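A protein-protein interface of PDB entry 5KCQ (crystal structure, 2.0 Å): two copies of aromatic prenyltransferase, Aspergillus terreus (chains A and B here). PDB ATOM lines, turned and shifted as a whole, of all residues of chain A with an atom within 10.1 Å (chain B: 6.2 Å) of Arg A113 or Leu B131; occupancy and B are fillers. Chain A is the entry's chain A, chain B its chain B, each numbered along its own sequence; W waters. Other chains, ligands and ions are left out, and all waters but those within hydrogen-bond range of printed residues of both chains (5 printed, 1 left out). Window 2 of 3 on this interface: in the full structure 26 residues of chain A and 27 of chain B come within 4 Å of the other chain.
No position is printed for both chains. Of the 10 pairs that touch across the chains among the printed residues, none has its exchanged pair printed and touching as well.
Hydrophobic or aromatic side chains of chain B that line the printed part of chain A: Ala B129 and Pro B133. Along chain B the printed residues that touch a printed residue of chain A span positions 126 to 133. Of the 23 printed residues of chain A, 4 touch a printed residue of chain B. Hydrophobic or aromatic side chains of chain A that line the printed part of chain B: Leu A108 and Phe A119. Among the printed residues, 10 pairs touch across the chains. Among the printed residues, no Asp or Glu carboxylate lies within 4 Å of a Lys or Arg side-chain nitrogen of the other chain.
The backbone carbonyl oxygen (O) of Leu A108 is in hydrogen-bond range of the side-chain hydroxyl (OG1) of Thr A111 (2.6 Å). The side-chain hydroxyl of Thr B130 is in hydrogen-bond range of the backbone carbonyl oxygen of Asn B127 (3.2 Å).
NH1 of Arg A113 is in hydrogen-bond range of O of Leu B131 (3.5 Å). The guanidinium group of Arg A151 lies within hydrogen-bond range of the backbone carbonyl oxygen of Thr B130, 3.2 Å away. The guanidinium group of Arg A113 sits at hydrogen-bond distance from the backbone carbonyl oxygen of Thr B130 (3.0 Å). The guanidinium group of Arg A151 sits at hydrogen-bond distance from the backbone carbonyl oxygen of Ala B129, at 2.9 Å.
Of the printed residues of chain B, Arg A113 touches Thr B130 and Leu B131. Of the printed residues of chain B, Phe A119 touches Lys B126 (3.8 Å), Ala B129 (3.8 Å) and Thr B130 (3.8 Å). Of the printed residues of chain A, Lys B126 touches Phe A119. Leu B131 touches just one residue of chain A: Arg A113 (3.5 Å). Leu B132 touches just one residue of chain A: Arg A151. The nearest residue of chain B that does not touch Arg A113 is Ala B129 (4.4 Å). The nearest printed residue of chain B that does not touch Phe A119 is Asn B127 (6.6 Å).
Water W2 lies within hydrogen-bond range of the backbone carbonyl oxygen (O) of Arg A113, the backbone carbonyl oxygen (O) of Ala B129 and the guanidinium group (NE) of Arg A151. Water W4 lies within hydrogen-bond range of the backbone NH (N) of Arg A151 (2.7 Å) and the backbone carbonyl oxygen (O) of Pro B133 (3.0 Å). Water W1 bridges NH2 of Arg A113 (2.8 Å) and O of Leu B131 (3.4 Å). Water W5 lies within hydrogen-bond range of the guanidinium group of Arg A151, the backbone carbonyl oxygen of Leu B131 and the guanidinium group of Arg A113. Water W3 lies within hydrogen-bond range of the backbone NH of Ala A152 (2.9 Å), the backbone carbonyl oxygen of Pro B133 (3.0 Å) and the backbone NH of Arg A151 (3.4 Å).
Among the printed residues, merely in contact across the chains: Leu A108 with Thr B130 (3.97 Å), Phe A119 with Lys B126 (3.8 Å), Phe A119 with Ala B129 (3.8 Å), Phe A119 with Thr B130 (3.8 Å), Arg A151 with Leu B132 (3.6 Å) and Arg A151 with Pro B133 (3.6 Å).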
ATOM      1  N   GLU A  73     -22.019   7.158 -14.164  1.00  0.00           N
ATOM      2  CA  GLU A  73     -21.063   6.455 -15.004  1.00  0.00           C
ATOM      3  C   GLU A  73     -21.738   5.662 -16.151  1.00  0.00           C
ATOM      4  O   GLU A  73     -21.112   5.400 -17.127  1.00  0.00           O
ATOM      5  CB  GLU A  73     -20.218   5.465 -14.149  1.00  0.00           C
ATOM      6  CG  GLU A  73     -19.518   6.101 -12.944  1.00  0.00           C
ATOM      7  CD  GLU A  73     -18.516   7.174 -13.355  1.00  0.00           C
ATOM      8  OE1 GLU A  73     -17.899   7.034 -14.385  1.00  0.00           O
ATOM      9  OE2 GLU A  73     -18.363   8.196 -12.658  1.00  0.00           O
ATOM     10  N   GLY A 106     -26.199  -2.179 -12.367  1.00  0.00           N
ATOM     11  CA  GLY A 106     -25.348  -2.596 -11.250  1.00  0.00           C
ATOM     12  C   GLY A 106     -24.597  -1.396 -10.696  1.00  0.00           C
ATOM     13  O   GLY A 106     -24.417  -0.373 -11.422  1.00  0.00           O
ATOM     14  N   PRO A 107     -24.117  -1.506  -9.451  1.00  0.00           N
ATOM     15  CA  PRO A 107     -23.409  -0.484  -8.779  1.00  0.00           C
ATOM     16  C   PRO A 107     -21.966  -0.187  -9.323  1.00  0.00           C
ATOM     17  O   PRO A 107     -21.343   0.772  -8.917  1.00  0.00           O
ATOM     18  CB  PRO A 107     -23.439  -0.969  -7.321  1.00  0.00           C
ATOM     19  CG  PRO A 107     -23.375  -2.422  -7.412  1.00  0.00           C
ATOM     20  CD  PRO A 107     -24.220  -2.735  -8.623  1.00  0.00           C
ATOM     21  N   LEU A 108     -21.436  -0.995 -10.205  1.00  0.00           N
ATOM     22  CA  LEU A 108     -20.146  -0.663 -10.875  1.00  0.00           C
ATOM     23  C   LEU A 108     -20.343  -0.500 -12.411  1.00  0.00           C
ATOM     24  O   LEU A 108     -19.373  -0.415 -13.197  1.00  0.00           O
ATOM     25  CB  LEU A 108     -19.126  -1.776 -10.597  1.00  0.00           C
ATOM     26  CG  LEU A 108     -18.723  -1.830  -9.128  1.00  0.00           C
ATOM     27  CD1 LEU A 108     -18.157  -3.150  -8.646  1.00  0.00           C
ATOM     28  CD2 LEU A 108     -17.755  -0.767  -8.809  1.00  0.00           C
ATOM     29  N   ALA A 109     -21.619  -0.453 -12.839  1.00  0.00           N
ATOM     30  CA  ALA A 109     -21.906  -0.325 -14.256  1.00  0.00           C
ATOM     31  C   ALA A 109     -21.144   0.830 -14.913  1.00  0.00           C
ATOM     32  O   ALA A 109     -21.034   1.890 -14.341  1.00  0.00           O
ATOM     33  CB  ALA A 109     -23.396  -0.175 -14.471  1.00  0.00           C
ATOM     34  N   GLY A 110     -20.720   0.632 -16.147  1.00  0.00           N
ATOM     35  CA  GLY A 110     -20.016   1.686 -16.932  1.00  0.00           C
ATOM     36  C   GLY A 110     -18.598   2.010 -16.400  1.00  0.00           C
ATOM     37  O   GLY A 110     -18.049   3.032 -16.783  1.00  0.00           O
ATOM     38  N   THR A 111     -18.015   1.160 -15.555  1.00  0.00           N
ATOM     39  CA  THR A 111     -16.651   1.302 -15.097  1.00  0.00           C
ATOM     40  C   THR A 111     -15.897   0.026 -15.437  1.00  0.00           C
ATOM     41  O   THR A 111     -16.501  -0.950 -15.931  1.00  0.00           O
ATOM     42  CB  THR A 111     -16.566   1.577 -13.603  1.00  0.00           C
ATOM     43  OG1 THR A 111     -16.904   0.375 -12.810  1.00  0.00           O
ATOM     44  CG2 THR A 111     -17.518   2.747 -13.296  1.00  0.00           C
ATOM     45  N   ALA A 112     -14.600   0.018 -15.166  1.00  0.00           N
ATOM     46  CA  ALA A 112     -13.746  -1.148 -15.561  1.00  0.00           C
ATOM     47  C   ALA A 112     -14.246  -2.531 -15.073  1.00  0.00           C
ATOM     48  O   ALA A 112     -14.101  -3.559 -15.766  1.00  0.00           O
ATOM     49  CB  ALA A 112     -12.264  -0.922 -15.240  1.00  0.00           C
ATOM     50  N   ARG A 113     -14.848  -2.562 -13.889  1.00  0.00           N
ATOM     51  CA  ARG A 113     -15.311  -3.831 -13.348  1.00  0.00           C
ATOM     52  C   ARG A 113     -16.630  -4.307 -13.934  1.00  0.00           C
ATOM     53  O   ARG A 113     -16.982  -5.424 -13.686  1.00  0.00           O
ATOM     54  CB  ARG A 113     -15.417  -3.819 -11.823  1.00  0.00           C
ATOM     55  CG  ARG A 113     -14.077  -3.677 -11.053  1.00  0.00           C
ATOM     56  CD  ARG A 113     -14.328  -3.325  -9.572  1.00  0.00           C
ATOM     57  NE  ARG A 113     -13.069  -3.019  -8.885  1.00  0.00           N
ATOM     58  CZ  ARG A 113     -12.238  -3.929  -8.410  1.00  0.00           C
ATOM     59  NH1 ARG A 113     -12.602  -5.191  -8.304  1.00  0.00           N
ATOM     60  NH2 ARG A 113     -11.065  -3.564  -7.917  1.00  0.00           N
ATOM     61  N   ASP A 114     -17.333  -3.473 -14.702  1.00  0.00           N
ATOM     62  CA  ASP A 114     -18.575  -3.882 -15.365  1.00  0.00           C
ATOM     63  C   ASP A 114     -18.867  -2.980 -16.564  1.00  0.00           C
ATOM     64  O   ASP A 114     -19.770  -2.126 -16.489  1.00  0.00           O
ATOM     65  CB  ASP A 114     -19.713  -3.823 -14.301  1.00  0.00           C
ATOM     66  CG  ASP A 114     -21.054  -4.309 -14.829  1.00  0.00           C
ATOM     67  OD1 ASP A 114     -21.059  -4.917 -15.925  1.00  0.00           O
ATOM     68  OD2 ASP A 114     -22.090  -4.076 -14.124  1.00  0.00           O
ATOM     69  N   PRO A 115     -18.057  -3.069 -17.634  1.00  0.00           N
ATOM     70  CA  PRO A 115     -18.196  -1.990 -18.683  1.00  0.00           C
ATOM     71  C   PRO A 115     -19.527  -1.985 -19.441  1.00  0.00           C
ATOM     72  O   PRO A 115     -20.009  -0.923 -19.818  1.00  0.00           O
ATOM     73  CB  PRO A 115     -16.948  -2.188 -19.552  1.00  0.00           C
ATOM     74  CG  PRO A 115     -16.055  -3.027 -18.719  1.00  0.00           C
ATOM     75  CD  PRO A 115     -16.883  -3.905 -17.878  1.00  0.00           C
ATOM     76  N   LEU A 116     -20.204  -3.145 -19.562  1.00  0.00           N
ATOM     77  CA  LEU A 116     -21.462  -3.204 -20.304  1.00  0.00           C
ATOM     78  C   LEU A 116     -22.720  -3.511 -19.469  1.00  0.00           C
ATOM     79  O   LEU A 116     -23.782  -3.880 -20.020  1.00  0.00           O
ATOM     80  CB  LEU A 116     -21.351  -4.260 -21.399  1.00  0.00           C
ATOM     81  CG  LEU A 116     -20.426  -3.985 -22.590  1.00  0.00           C
ATOM     82  CD1 LEU A 116     -20.612  -5.101 -23.603  1.00  0.00           C
ATOM     83  CD2 LEU A 116     -20.669  -2.612 -23.225  1.00  0.00           C
ATOM     84  N   ASN A 117     -22.619  -3.294 -18.158  1.00  0.00           N
ATOM     85  CA  ASN A 117     -23.713  -3.535 -17.187  1.00  0.00           C
ATOM     86  C   ASN A 117     -24.254  -4.923 -17.335  1.00  0.00           C
ATOM     87  O   ASN A 117     -25.450  -5.129 -17.665  1.00  0.00           O
ATOM     88  CB  ASN A 117     -24.865  -2.528 -17.363  1.00  0.00           C
ATOM     89  CG  ASN A 117     -25.869  -2.645 -16.262  1.00  0.00           C
ATOM     90  OD1 ASN A 117     -25.499  -2.690 -15.062  1.00  0.00           O
ATOM     91  ND2 ASN A 117     -27.132  -2.758 -16.625  1.00  0.00           N
ATOM     92  N   SER A 118     -23.376  -5.890 -17.179  1.00  0.00           N
ATOM     93  CA  SER A 118     -23.675  -7.327 -17.535  1.00  0.00           C
ATOM     94  C   SER A 118     -24.368  -8.159 -16.472  1.00  0.00           C
ATOM     95  O   SER A 118     -24.750  -9.284 -16.746  1.00  0.00           O
ATOM     96  CB  SER A 118     -22.347  -8.056 -17.833  1.00  0.00           C
ATOM     97  OG  SER A 118     -21.798  -7.487 -19.013  1.00  0.00           O
ATOM     98  N   PHE A 119     -24.545  -7.626 -15.267  1.00  0.00           N
ATOM     99  CA  PHE A 119     -25.038  -8.437 -14.098  1.00  0.00           C
ATOM    100  C   PHE A 119     -26.369  -7.981 -13.502  1.00  0.00           C
ATOM    101  O   PHE A 119     -27.066  -8.808 -12.870  1.00  0.00           O
ATOM    102  CB  PHE A 119     -23.979  -8.463 -12.965  1.00  0.00           C
ATOM    103  CG  PHE A 119     -22.632  -8.781 -13.482  1.00  0.00           C
ATOM    104  CD1 PHE A 119     -22.357 -10.036 -14.009  1.00  0.00           C
ATOM    105  CD2 PHE A 119     -21.697  -7.772 -13.619  1.00  0.00           C
ATOM    106  CE1 PHE A 119     -21.101 -10.317 -14.587  1.00  0.00           C
ATOM    107  CE2 PHE A 119     -20.438  -8.029 -14.181  1.00  0.00           C
ATOM    108  CZ  PHE A 119     -20.152  -9.305 -14.695  1.00  0.00           C
ATOM    109  N   GLY A 120     -26.714  -6.690 -13.616  1.00  0.00           N
ATOM    110  CA  GLY A 120     -27.869  -6.170 -12.853  1.00  0.00           C
ATOM    111  C   GLY A 120     -29.172  -6.840 -13.274  1.00  0.00           C
ATOM    112  O   GLY A 120     -30.019  -7.154 -12.404  1.00  0.00           O
ATOM    113  N   LEU A 149     -20.441 -11.403 -22.822  1.00  0.00           N
ATOM    114  CA  LEU A 149     -19.050 -11.258 -23.063  1.00  0.00           C
ATOM    115  C   LEU A 149     -18.357 -11.230 -21.715  1.00  0.00           C
ATOM    116  O   LEU A 149     -18.933 -10.732 -20.742  1.00  0.00           O
ATOM    117  CB  LEU A 149     -18.783  -9.923 -23.762  1.00  0.00           C
ATOM    118  CG  LEU A 149     -19.330  -9.724 -25.163  1.00  0.00           C
ATOM    119  CD1 LEU A 149     -18.996  -8.336 -25.648  1.00  0.00           C
ATOM    120  CD2 LEU A 149     -18.703 -10.787 -26.052  1.00  0.00           C
ATOM    121  N   ASP A 150     -17.099 -11.664 -21.696  1.00  0.00           N
ATOM    122  CA  ASP A 150     -16.276 -11.474 -20.486  1.00  0.00           C
ATOM    123  C   ASP A 150     -15.790 -10.032 -20.314  1.00  0.00           C
ATOM    124  O   ASP A 150     -16.033  -9.141 -21.168  1.00  0.00           O
ATOM    125  CB  ASP A 150     -15.150 -12.521 -20.420  1.00  0.00           C
ATOM    126  CG  ASP A 150     -14.005 -12.222 -21.372  1.00  0.00           C
ATOM    127  OD1 ASP A 150     -13.866 -11.103 -21.884  1.00  0.00           O
ATOM    128  OD2 ASP A 150     -13.210 -13.109 -21.567  1.00  0.00           O
ATOM    129  N   ARG A 151     -15.104  -9.762 -19.189  1.00  0.00           N
ATOM    130  CA  ARG A 151     -14.788  -8.367 -18.867  1.00  0.00           C
ATOM    131  C   ARG A 151     -13.937  -7.748 -19.938  1.00  0.00           C
ATOM    132  O   ARG A 151     -14.228  -6.663 -20.395  1.00  0.00           O
ATOM    133  CB  ARG A 151     -14.101  -8.195 -17.493  1.00  0.00           C
ATOM    134  CG  ARG A 151     -13.868  -6.737 -17.136  1.00  0.00           C
ATOM    135  CD  ARG A 151     -12.971  -6.586 -15.895  1.00  0.00           C
ATOM    136  NE  ARG A 151     -13.614  -7.155 -14.716  1.00  0.00           N
ATOM    137  CZ  ARG A 151     -13.138  -7.069 -13.466  1.00  0.00           C
ATOM    138  NH1 ARG A 151     -12.081  -6.377 -13.229  1.00  0.00           N
ATOM    139  NH2 ARG A 151     -13.790  -7.603 -12.453  1.00  0.00           N
ATOM    140  N   ALA A 152     -12.882  -8.437 -20.351  1.00  0.00           N
ATOM    141  CA  ALA A 152     -11.944  -7.850 -21.366  1.00  0.00           C
ATOM    142  C   ALA A 152     -12.687  -7.560 -22.709  1.00  0.00           C
ATOM    143  O   ALA A 152     -12.473  -6.522 -23.347  1.00  0.00           O
ATOM    144  CB  ALA A 152     -10.777  -8.831 -21.618  1.00  0.00           C
ATOM    145  N   CYS A 154     -15.928  -6.995 -22.989  1.00  0.00           N
ATOM    146  CA  CYS A 154     -16.824  -5.877 -22.680  1.00  0.00           C
ATOM    147  C   CYS A 154     -16.032  -4.557 -22.799  1.00  0.00           C
ATOM    148  O   CYS A 154     -16.528  -3.582 -23.409  1.00  0.00           O
ATOM    149  CB  CYS A 154     -17.413  -5.934 -21.291  1.00  0.00           C
ATOM    150  SG  CYS A 154     -18.682  -7.205 -21.070  1.00  0.00           S
ATOM    151  N   ALA A 155     -14.807  -4.537 -22.277  1.00  0.00           N
ATOM    152  CA  ALA A 155     -13.972  -3.329 -22.426  1.00  0.00           C
ATOM    153  C   ALA A 155     -13.669  -3.056 -23.893  1.00  0.00           C
ATOM    154  O   ALA A 155     -13.732  -1.911 -24.305  1.00  0.00           O
ATOM    155  CB  ALA A 155     -12.651  -3.431 -21.650  1.00  0.00           C
ATOM    156  N   THR A 158     -16.696  -1.473 -25.517  1.00  0.00           N
ATOM    157  CA  THR A 158     -16.936  -0.062 -25.182  1.00  0.00           C
ATOM    158  C   THR A 158     -16.143   0.916 -26.030  1.00  0.00           C
ATOM    159  O   THR A 158     -16.628   2.011 -26.281  1.00  0.00           O
ATOM    160  CB  THR A 158     -16.664   0.281 -23.703  1.00  0.00           C
ATOM    161  OG1 THR A 158     -15.292   0.050 -23.416  1.00  0.00           O
ATOM    162  CG2 THR A 158     -17.575  -0.510 -22.773  1.00  0.00           C
ATOM    163  N   PHE B  53     -10.898 -12.251   1.746  1.00  0.00           N
ATOM    164  CA  PHE B  53     -11.830 -12.752   0.753  1.00  0.00           C
ATOM    165  C   PHE B  53     -12.897 -13.704   1.354  1.00  0.00           C
ATOM    166  O   PHE B  53     -14.139 -13.588   1.041  1.00  0.00           O
ATOM    167  CB  PHE B  53     -11.033 -13.460  -0.366  1.00  0.00           C
ATOM    168  CG  PHE B  53     -11.907 -14.237  -1.279  1.00  0.00           C
ATOM    169  CD1 PHE B  53     -12.614 -13.610  -2.232  1.00  0.00           C
ATOM    170  CD2 PHE B  53     -12.049 -15.591  -1.119  1.00  0.00           C
ATOM    171  CE1 PHE B  53     -13.471 -14.338  -3.081  1.00  0.00           C
ATOM    172  CE2 PHE B  53     -12.846 -16.306  -1.947  1.00  0.00           C
ATOM    173  CZ  PHE B  53     -13.566 -15.689  -2.918  1.00  0.00           C
ATOM    174  N   TYR B  57     -16.772 -12.612   1.184  1.00  0.00           N
ATOM    175  CA  TYR B  57     -17.544 -13.330   0.157  1.00  0.00           C
ATOM    176  C   TYR B  57     -18.109 -14.654   0.565  1.00  0.00           C
ATOM    177  O   TYR B  57     -19.197 -15.038   0.083  1.00  0.00           O
ATOM    178  CB  TYR B  57     -16.723 -13.466  -1.143  1.00  0.00           C
ATOM    179  CG  TYR B  57     -16.525 -12.141  -1.778  1.00  0.00           C
ATOM    180  CD1 TYR B  57     -17.539 -11.558  -2.482  1.00  0.00           C
ATOM    181  CD2 TYR B  57     -15.376 -11.352  -1.532  1.00  0.00           C
ATOM    182  CE1 TYR B  57     -17.385 -10.301  -3.044  1.00  0.00           C
ATOM    183  CE2 TYR B  57     -15.237 -10.097  -2.055  1.00  0.00           C
ATOM    184  CZ  TYR B  57     -16.246  -9.571  -2.814  1.00  0.00           C
ATOM    185  OH  TYR B  57     -16.193  -8.358  -3.410  1.00  0.00           O
ATOM    186  N   LYS B 126     -21.511 -13.919  -9.536  1.00  0.00           N
ATOM    187  CA  LYS B 126     -21.622 -12.513  -9.977  1.00  0.00           C
ATOM    188  C   LYS B 126     -20.755 -11.554  -9.158  1.00  0.00           C
ATOM    189  O   LYS B 126     -20.069 -10.681  -9.730  1.00  0.00           O
ATOM    190  CB  LYS B 126     -23.066 -12.009  -9.843  1.00  0.00           C
ATOM    191  CG  LYS B 126     -23.231 -10.470  -9.868  1.00  0.00           C
ATOM    192  CD  LYS B 126     -24.528 -10.053  -9.173  1.00  0.00           C
ATOM    193  CE  LYS B 126     -24.343  -9.363  -7.844  1.00  0.00           C
ATOM    194  NZ  LYS B 126     -25.526  -9.563  -6.996  1.00  0.00           N
ATOM    195  N   ASN B 127     -20.768 -11.692  -7.849  1.00  0.00           N
ATOM    196  CA  ASN B 127     -19.831 -10.869  -7.028  1.00  0.00           C
ATOM    197  C   ASN B 127     -18.374 -11.159  -7.295  1.00  0.00           C
ATOM    198  O   ASN B 127     -17.554 -10.246  -7.336  1.00  0.00           O
ATOM    199  CB  ASN B 127     -20.155 -11.003  -5.584  1.00  0.00           C
ATOM    200  CG  ASN B 127     -21.465 -10.338  -5.251  1.00  0.00           C
ATOM    201  OD1 ASN B 127     -21.792  -9.299  -5.791  1.00  0.00           O
ATOM    202  ND2 ASN B 127     -22.240 -10.991  -4.482  1.00  0.00           N
ATOM    203  N   LEU B 128     -18.049 -12.389  -7.628  1.00  0.00           N
ATOM    204  CA  LEU B 128     -16.678 -12.667  -8.021  1.00  0.00           C
ATOM    205  C   LEU B 128     -16.296 -12.054  -9.382  1.00  0.00           C
ATOM    206  O   LEU B 128     -15.128 -11.767  -9.609  1.00  0.00           O
ATOM    207  CB  LEU B 128     -16.384 -14.204  -8.039  1.00  0.00           C
ATOM    208  CG  LEU B 128     -16.632 -14.973  -6.755  1.00  0.00           C
ATOM    209  CD1 LEU B 128     -16.237 -16.452  -6.828  1.00  0.00           C
ATOM    210  CD2 LEU B 128     -16.028 -14.248  -5.535  1.00  0.00           C
ATOM    211  N   ALA B 129     -17.284 -11.952 -10.305  1.00  0.00           N
ATOM    212  CA  ALA B 129     -17.019 -11.469 -11.641  1.00  0.00           C
ATOM    213  C   ALA B 129     -16.744  -9.962 -11.603  1.00  0.00           C
ATOM    214  O   ALA B 129     -16.025  -9.509 -12.418  1.00  0.00           O
ATOM    215  CB  ALA B 129     -18.169 -11.806 -12.562  1.00  0.00           C
ATOM    216  N   THR B 130     -17.252  -9.200 -10.624  1.00  0.00           N
ATOM    217  CA  THR B 130     -16.796  -7.832 -10.456  1.00  0.00           C
ATOM    218  C   THR B 130     -15.566  -7.686  -9.552  1.00  0.00           C
ATOM    219  O   THR B 130     -14.911  -6.653  -9.571  1.00  0.00           O
ATOM    220  CB  THR B 130     -17.883  -6.905  -9.911  1.00  0.00           C
ATOM    221  OG1 THR B 130     -18.361  -7.442  -8.720  1.00  0.00           O
ATOM    222  CG2 THR B 130     -19.027  -6.805 -10.865  1.00  0.00           C
ATOM    223  N   LEU B 131     -15.248  -8.716  -8.782  1.00  0.00           N
ATOM    224  CA  LEU B 131     -14.015  -8.761  -7.998  1.00  0.00           C
ATOM    225  C   LEU B 131     -12.757  -9.118  -8.804  1.00  0.00           C
ATOM    226  O   LEU B 131     -11.716  -8.520  -8.629  1.00  0.00           O
ATOM    227  CB  LEU B 131     -14.170  -9.785  -6.894  1.00  0.00           C
ATOM    228  CG  LEU B 131     -12.965 -10.022  -5.971  1.00  0.00           C
ATOM    229  CD1 LEU B 131     -12.662  -8.803  -5.158  1.00  0.00           C
ATOM    230  CD2 LEU B 131     -13.160 -11.222  -5.091  1.00  0.00           C
ATOM    231  N   LEU B 132     -12.858 -10.169  -9.610  1.00  0.00           N
ATOM    232  CA  LEU B 132     -11.731 -10.830 -10.252  1.00  0.00           C
ATOM    233  C   LEU B 132     -11.831 -10.672 -11.799  1.00  0.00           C
ATOM    234  O   LEU B 132     -12.817 -11.028 -12.393  1.00  0.00           O
ATOM    235  CB  LEU B 132     -11.789 -12.281  -9.911  1.00  0.00           C
ATOM    236  CG  LEU B 132     -11.861 -12.708  -8.442  1.00  0.00           C
ATOM    237  CD1 LEU B 132     -12.416 -14.110  -8.310  1.00  0.00           C
ATOM    238  CD2 LEU B 132     -10.488 -12.607  -7.775  1.00  0.00           C
ATOM    239  N   PRO B 133     -10.779 -10.181 -12.457  1.00  0.00           N
ATOM    240  CA  PRO B 133     -10.897  -9.901 -13.914  1.00  0.00           C
ATOM    241  C   PRO B 133     -11.065 -11.122 -14.797  1.00  0.00           C
ATOM    242  O   PRO B 133     -11.550 -10.992 -15.902  1.00  0.00           O
ATOM    243  CB  PRO B 133      -9.581  -9.201 -14.261  1.00  0.00           C
ATOM    244  CG  PRO B 133      -8.635  -9.533 -13.147  1.00  0.00           C
ATOM    245  CD  PRO B 133      -9.442  -9.910 -11.925  1.00  0.00           C
ATOM    246  N   VAL B 180      -7.969 -16.488  -7.069  1.00  0.00           N
ATOM    247  CA  VAL B 180      -9.104 -17.327  -6.705  1.00  0.00           C
ATOM    248  C   VAL B 180      -9.687 -17.825  -8.027  1.00  0.00           C
ATOM    249  O   VAL B 180     -10.064 -17.042  -8.885  1.00  0.00           O
ATOM    250  CB  VAL B 180     -10.151 -16.543  -5.910  1.00  0.00           C
ATOM    251  CG1 VAL B 180     -11.362 -17.360  -5.643  1.00  0.00           C
ATOM    252  CG2 VAL B 180      -9.506 -16.047  -4.618  1.00  0.00           C
HETATM  253  O   HOH W   1     -10.370  -6.009  -6.865  1.00  0.00           O
HETATM  254  O   HOH W   2     -16.583  -7.833 -14.891  1.00  0.00           O
HETATM  255  O   HOH W   3     -11.855 -10.698 -18.839  1.00  0.00           O
HETATM  256  O   HOH W   4     -14.152 -11.409 -17.235  1.00  0.00           O
HETATM  257  O   HOH W   5     -10.832  -6.840 -10.792  1.00  0.00           O
